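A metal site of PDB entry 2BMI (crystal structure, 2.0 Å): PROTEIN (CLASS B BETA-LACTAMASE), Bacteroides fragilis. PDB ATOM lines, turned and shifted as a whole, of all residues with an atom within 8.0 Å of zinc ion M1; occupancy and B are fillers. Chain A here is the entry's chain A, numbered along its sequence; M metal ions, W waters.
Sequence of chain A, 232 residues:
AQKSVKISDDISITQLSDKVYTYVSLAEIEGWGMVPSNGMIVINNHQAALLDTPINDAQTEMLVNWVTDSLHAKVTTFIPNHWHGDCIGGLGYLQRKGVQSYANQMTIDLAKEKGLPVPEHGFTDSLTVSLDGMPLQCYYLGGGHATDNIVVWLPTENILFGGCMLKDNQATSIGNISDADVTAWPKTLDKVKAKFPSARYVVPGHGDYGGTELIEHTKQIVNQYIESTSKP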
ATOM      1  N   VAL A  35       5.627 -28.521 -14.287  1.00  0.00           N
ATOM      2  CA  VAL A  35       4.698 -28.623 -13.180  1.00  0.00           C
ATOM      3  C   VAL A  35       3.364 -28.016 -13.629  1.00  0.00           C
ATOM      4  O   VAL A  35       3.347 -26.919 -14.182  1.00  0.00           O
ATOM      5  CB  VAL A  35       5.252 -27.900 -11.932  1.00  0.00           C
ATOM      6  CG1 VAL A  35       4.255 -27.993 -10.806  1.00  0.00           C
ATOM      7  CG2 VAL A  35       6.574 -28.546 -11.490  1.00  0.00           C
ATOM      8  N   PRO A  36       2.254 -28.762 -13.486  1.00  0.00           N
ATOM      9  CA  PRO A  36       0.928 -28.250 -13.876  1.00  0.00           C
ATOM     10  C   PRO A  36       0.308 -27.479 -12.725  1.00  0.00           C
ATOM     11  O   PRO A  36       0.508 -27.820 -11.556  1.00  0.00           O
ATOM     12  CB  PRO A  36       0.157 -29.525 -14.139  1.00  0.00           C
ATOM     13  CG  PRO A  36       0.622 -30.417 -13.035  1.00  0.00           C
ATOM     14  CD  PRO A  36       2.153 -30.176 -13.058  1.00  0.00           C
ATOM     15  N   SER A  37      -0.356 -26.375 -13.044  1.00  0.00           N
ATOM     16  CA  SER A  37      -1.031 -25.596 -12.015  1.00  0.00           C
ATOM     17  C   SER A  37      -2.467 -25.385 -12.470  1.00  0.00           C
ATOM     18  O   SER A  37      -2.753 -25.396 -13.666  1.00  0.00           O
ATOM     19  CB  SER A  37      -0.277 -24.284 -11.682  1.00  0.00           C
ATOM     20  OG  SER A  37      -0.101 -23.483 -12.826  1.00  0.00           O
ATOM     21  N   ASN A  38      -3.378 -25.266 -11.500  1.00  0.00           N
ATOM     22  CA  ASN A  38      -4.812 -25.129 -11.796  1.00  0.00           C
ATOM     23  C   ASN A  38      -5.387 -23.763 -11.545  1.00  0.00           C
ATOM     24  O   ASN A  38      -4.928 -23.027 -10.682  1.00  0.00           O
ATOM     25  CB  ASN A  38      -5.603 -26.096 -10.929  1.00  0.00           C
ATOM     26  CG  ASN A  38      -5.218 -27.541 -11.134  1.00  0.00           C
ATOM     27  OD1 ASN A  38      -4.857 -27.976 -12.232  1.00  0.00           O
ATOM     28  ND2 ASN A  38      -5.353 -28.326 -10.066  1.00  0.00           N
ATOM     29  N   ASP A  52      -6.912 -17.379 -10.273  1.00  0.00           N
ATOM     30  CA  ASP A  52      -5.507 -17.772 -10.475  1.00  0.00           C
ATOM     31  C   ASP A  52      -5.123 -17.662 -11.946  1.00  0.00           C
ATOM     32  O   ASP A  52      -5.916 -17.994 -12.848  1.00  0.00           O
ATOM     33  CB  ASP A  52      -5.235 -19.223 -10.036  1.00  0.00           C
ATOM     34  CG  ASP A  52      -4.927 -19.353  -8.544  1.00  0.00           C
ATOM     35  OD1 ASP A  52      -5.338 -18.467  -7.756  1.00  0.00           O
ATOM     36  OD2 ASP A  52      -4.291 -20.371  -8.158  1.00  0.00           O
ATOM     37  N   ILE A  55       1.488 -19.463 -14.952  1.00  0.00           N
ATOM     38  CA  ILE A  55       2.745 -18.952 -14.437  1.00  0.00           C
ATOM     39  C   ILE A  55       3.303 -17.670 -15.084  1.00  0.00           C
ATOM     40  O   ILE A  55       4.125 -16.966 -14.471  1.00  0.00           O
ATOM     41  CB  ILE A  55       3.810 -20.108 -14.406  1.00  0.00           C
ATOM     42  CG1 ILE A  55       4.069 -20.513 -12.968  1.00  0.00           C
ATOM     43  CG2 ILE A  55       5.083 -19.792 -15.179  1.00  0.00           C
ATOM     44  CD1 ILE A  55       2.961 -21.332 -12.454  1.00  0.00           C
ATOM     45  N   ASN A  81      -5.231 -17.108  -5.521  1.00  0.00           N
ATOM     46  CA  ASN A  81      -5.290 -17.856  -4.280  1.00  0.00           C
ATOM     47  C   ASN A  81      -4.296 -17.317  -3.275  1.00  0.00           C
ATOM     48  O   ASN A  81      -4.553 -17.252  -2.076  1.00  0.00           O
ATOM     49  CB  ASN A  81      -5.011 -19.334  -4.499  1.00  0.00           C
ATOM     50  CG  ASN A  81      -5.257 -20.155  -3.255  1.00  0.00           C
ATOM     51  OD1 ASN A  81      -4.310 -20.560  -2.581  1.00  0.00           O
ATOM     52  ND2 ASN A  81      -6.522 -20.379  -2.930  1.00  0.00           N
ATOM     53  N   HIS A  82      -3.104 -17.005  -3.767  1.00  0.00           N
ATOM     54  CA  HIS A  82      -2.078 -16.415  -2.930  1.00  0.00           C
ATOM     55  C   HIS A  82      -1.037 -15.719  -3.776  1.00  0.00           C
ATOM     56  O   HIS A  82      -1.263 -15.502  -4.968  1.00  0.00           O
ATOM     57  CB  HIS A  82      -1.465 -17.431  -1.926  1.00  0.00           C
ATOM     58  CG  HIS A  82      -0.924 -18.675  -2.555  1.00  0.00           C
ATOM     59  ND1 HIS A  82      -1.716 -19.676  -3.063  1.00  0.00           N
ATOM     60  CD2 HIS A  82       0.359 -19.065  -2.739  1.00  0.00           C
ATOM     61  CE1 HIS A  82      -0.906 -20.617  -3.526  1.00  0.00           C
ATOM     62  NE2 HIS A  82       0.361 -20.286  -3.358  1.00  0.00           N
ATOM     63  N   HIS A  84       2.019 -16.681  -4.817  1.00  0.00           N
ATOM     64  CA  HIS A  84       2.919 -17.449  -5.687  1.00  0.00           C
ATOM     65  C   HIS A  84       2.671 -17.274  -7.192  1.00  0.00           C
ATOM     66  O   HIS A  84       1.594 -16.838  -7.613  1.00  0.00           O
ATOM     67  CB  HIS A  84       2.941 -18.922  -5.304  1.00  0.00           C
ATOM     68  CG  HIS A  84       3.682 -19.199  -4.039  1.00  0.00           C
ATOM     69  ND1 HIS A  84       3.482 -20.348  -3.298  1.00  0.00           N
ATOM     70  CD2 HIS A  84       4.590 -18.419  -3.407  1.00  0.00           C
ATOM     71  CE1 HIS A  84       4.259 -20.239  -2.246  1.00  0.00           C
ATOM     72  NE2 HIS A  84       4.953 -19.096  -2.256  1.00  0.00           N
ATOM     73  N   GLY A  85       3.669 -17.637  -7.986  1.00  0.00           N
ATOM     74  CA  GLY A  85       3.568 -17.480  -9.422  1.00  0.00           C
ATOM     75  C   GLY A  85       2.440 -18.225 -10.094  1.00  0.00           C
ATOM     76  O   GLY A  85       1.959 -17.817 -11.178  1.00  0.00           O
ATOM     77  N   ASP A  86       2.065 -19.354  -9.513  1.00  0.00           N
ATOM     78  CA  ASP A  86       0.972 -20.148 -10.056  1.00  0.00           C
ATOM     79  C   ASP A  86      -0.399 -19.555  -9.734  1.00  0.00           C
ATOM     80  O   ASP A  86      -1.433 -20.155 -10.074  1.00  0.00           O
ATOM     81  CB  ASP A  86       1.067 -21.635  -9.665  1.00  0.00           C
ATOM     82  CG  ASP A  86       1.304 -21.860  -8.198  1.00  0.00           C
ATOM     83  OD1 ASP A  86       2.178 -21.210  -7.619  1.00  0.00           O
ATOM     84  OD2 ASP A  86       0.634 -22.772  -7.636  1.00  0.00           O
ATOM     85  N   CYS A  87      -0.379 -18.359  -9.131  1.00  0.00           N
ATOM     86  CA  CYS A  87      -1.595 -17.609  -8.768  1.00  0.00           C
ATOM     87  C   CYS A  87      -1.594 -16.228  -9.437  1.00  0.00           C
ATOM     88  O   CYS A  87      -2.629 -15.794  -9.960  1.00  0.00           O
ATOM     89  CB  CYS A  87      -1.702 -17.422  -7.242  1.00  0.00           C
ATOM     90  SG  CYS A  87      -1.659 -18.951  -6.319  1.00  0.00           S
ATOM     91  N   HIS A 145      -0.728 -23.717   3.050  1.00  0.00           N
ATOM     92  CA  HIS A 145       0.341 -23.856   2.061  1.00  0.00           C
ATOM     93  C   HIS A 145       1.148 -22.538   1.970  1.00  0.00           C
ATOM     94  O   HIS A 145       2.342 -22.556   1.654  1.00  0.00           O
ATOM     95  CB  HIS A 145      -0.262 -24.203   0.712  1.00  0.00           C
ATOM     96  CG  HIS A 145       0.644 -23.916  -0.431  1.00  0.00           C
ATOM     97  ND1 HIS A 145       1.597 -24.804  -0.881  1.00  0.00           N
ATOM     98  CD2 HIS A 145       0.731 -22.826  -1.243  1.00  0.00           C
ATOM     99  CE1 HIS A 145       2.226 -24.244  -1.924  1.00  0.00           C
ATOM    100  NE2 HIS A 145       1.741 -23.032  -2.180  1.00  0.00           N
ATOM    101  N   GLY A 163      -7.648 -24.230  -3.840  1.00  0.00           N
ATOM    102  CA  GLY A 163      -6.298 -23.792  -4.122  1.00  0.00           C
ATOM    103  C   GLY A 163      -5.223 -24.716  -3.559  1.00  0.00           C
ATOM    104  O   GLY A 163      -5.487 -25.847  -3.155  1.00  0.00           O
ATOM    105  N   CYS A 164      -4.011 -24.178  -3.507  1.00  0.00           N
ATOM    106  CA  CYS A 164      -2.844 -24.899  -3.059  1.00  0.00           C
ATOM    107  C   CYS A 164      -2.831 -25.423  -1.641  1.00  0.00           C
ATOM    108  O   CYS A 164      -1.943 -26.200  -1.304  1.00  0.00           O
ATOM    109  CB  CYS A 164      -1.610 -24.069  -3.377  1.00  0.00           C
ATOM    110  SG  CYS A 164      -1.466 -23.715  -5.156  1.00  0.00           S
ATOM    111  N   MET A 165      -3.769 -25.000  -0.783  1.00  0.00           N
ATOM    112  CA  MET A 165      -3.808 -25.521   0.578  1.00  0.00           C
ATOM    113  C   MET A 165      -4.364 -26.935   0.574  1.00  0.00           C
ATOM    114  O   MET A 165      -4.340 -27.638   1.594  1.00  0.00           O
ATOM    115  CB  MET A 165      -4.695 -24.641   1.470  1.00  0.00           C
ATOM    116  CG  MET A 165      -6.195 -24.722   1.128  1.00  0.00           C
ATOM    117  SD  MET A 165      -7.153 -24.021   2.474  1.00  0.00           S
ATOM    118  CE  MET A 165      -6.754 -22.273   2.368  1.00  0.00           C
ATOM    119  N   LEU A 166      -4.881 -27.349  -0.575  1.00  0.00           N
ATOM    120  CA  LEU A 166      -5.448 -28.678  -0.741  1.00  0.00           C
ATOM    121  C   LEU A 166      -4.671 -29.444  -1.804  1.00  0.00           C
ATOM    122  O   LEU A 166      -4.257 -28.885  -2.816  1.00  0.00           O
ATOM    123  CB  LEU A 166      -6.913 -28.614  -1.202  1.00  0.00           C
ATOM    124  CG  LEU A 166      -7.979 -27.876  -0.389  1.00  0.00           C
ATOM    125  CD1 LEU A 166      -9.294 -28.052  -1.099  1.00  0.00           C
ATOM    126  CD2 LEU A 166      -8.044 -28.378   1.031  1.00  0.00           C
ATOM    127  N   LYS A 167      -4.521 -30.755  -1.573  1.00  0.00           N
ATOM    128  CA  LYS A 167      -3.795 -31.638  -2.479  1.00  0.00           C
ATOM    129  C   LYS A 167      -4.771 -32.577  -3.194  1.00  0.00           C
ATOM    130  O   LYS A 167      -5.868 -32.869  -2.675  1.00  0.00           O
ATOM    131  CB  LYS A 167      -2.770 -32.483  -1.687  1.00  0.00           C
ATOM    132  CG  LYS A 167      -1.753 -31.691  -0.841  1.00  0.00           C
ATOM    133  CD  LYS A 167      -0.690 -31.013  -1.709  1.00  0.00           C
ATOM    134  CE  LYS A 167       0.018 -32.069  -2.533  1.00  0.00           C
ATOM    135  NZ  LYS A 167       1.075 -31.537  -3.454  1.00  0.00           N
ATOM    136  N   ASN A 176       5.822 -27.953  -1.936  1.00  0.00           N
ATOM    137  CA  ASN A 176       6.553 -26.733  -1.598  1.00  0.00           C
ATOM    138  C   ASN A 176       6.081 -26.077  -0.340  1.00  0.00           C
ATOM    139  O   ASN A 176       5.028 -25.421  -0.351  1.00  0.00           O
ATOM    140  CB  ASN A 176       6.458 -25.717  -2.744  1.00  0.00           C
ATOM    141  CG  ASN A 176       7.181 -24.395  -2.419  1.00  0.00           C
ATOM    142  OD1 ASN A 176       8.188 -24.391  -1.708  1.00  0.00           O
ATOM    143  ND2 ASN A 176       6.674 -23.290  -2.958  1.00  0.00           N
ATOM    144  N   PRO A 204      -8.009 -28.473  -6.299  1.00  0.00           N
ATOM    145  CA  PRO A 204      -6.756 -28.168  -5.587  1.00  0.00           C
ATOM    146  C   PRO A 204      -5.882 -27.265  -6.480  1.00  0.00           C
ATOM    147  O   PRO A 204      -6.191 -27.066  -7.642  1.00  0.00           O
ATOM    148  CB  PRO A 204      -6.142 -29.544  -5.423  1.00  0.00           C
ATOM    149  CG  PRO A 204      -6.462 -30.174  -6.779  1.00  0.00           C
ATOM    150  CD  PRO A 204      -7.937 -29.788  -6.971  1.00  0.00           C
ATOM    151  N   GLY A 205      -4.788 -26.729  -5.921  1.00  0.00           N
ATOM    152  CA  GLY A 205      -3.903 -25.871  -6.702  1.00  0.00           C
ATOM    153  C   GLY A 205      -3.160 -26.612  -7.806  1.00  0.00           C
ATOM    154  O   GLY A 205      -2.819 -26.010  -8.820  1.00  0.00           O
ATOM    155  N   HIS A 206      -2.891 -27.905  -7.581  1.00  0.00           N
ATOM    156  CA  HIS A 206      -2.204 -28.774  -8.543  1.00  0.00           C
ATOM    157  C   HIS A 206      -2.865 -30.162  -8.475  1.00  0.00           C
ATOM    158  O   HIS A 206      -3.212 -30.641  -7.389  1.00  0.00           O
ATOM    159  CB  HIS A 206      -0.724 -28.907  -8.180  1.00  0.00           C
ATOM    160  CG  HIS A 206      -0.034 -27.585  -7.968  1.00  0.00           C
ATOM    161  ND1 HIS A 206       0.493 -26.827  -8.989  1.00  0.00           N
ATOM    162  CD2 HIS A 206       0.129 -26.853  -6.844  1.00  0.00           C
ATOM    163  CE1 HIS A 206       0.938 -25.675  -8.464  1.00  0.00           C
ATOM    164  NE2 HIS A 206       0.748 -25.633  -7.163  1.00  0.00           N
HETATM  165 ZN    ZN M   1       0.799 -24.053  -5.909  1.00  0.00          ZN
HETATM  166 ZN    ZN M   2       1.940 -21.674  -3.716  1.00  0.00          ZN
HETATM  167  O   HOH W   1       1.491 -25.455  -4.335  1.00  0.00           O
HETATM  168  O   HOH W   2       1.913 -22.755  -5.127  1.00  0.00           O
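Zinc ion M1 is bound by water W2 (1.9 Å). NE2 of His 206 binds zinc ion M1, 2.0 Å away. Zinc ion M1 is bound by OD2 of Asp 86 (2.2 Å). Zinc ion M1 is bound by water W1, 2.2 Å away. Zinc ion M1 is bound by SG of Cys 164 (2.4 Å).
Residues that only touch zinc ion M1: His 145. The nearest printed residue that does not touch zinc ion M1 is His 82 (4.5 Å).
O of Pro 36 is in hydrogen-bond range of ND1 of His 206.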
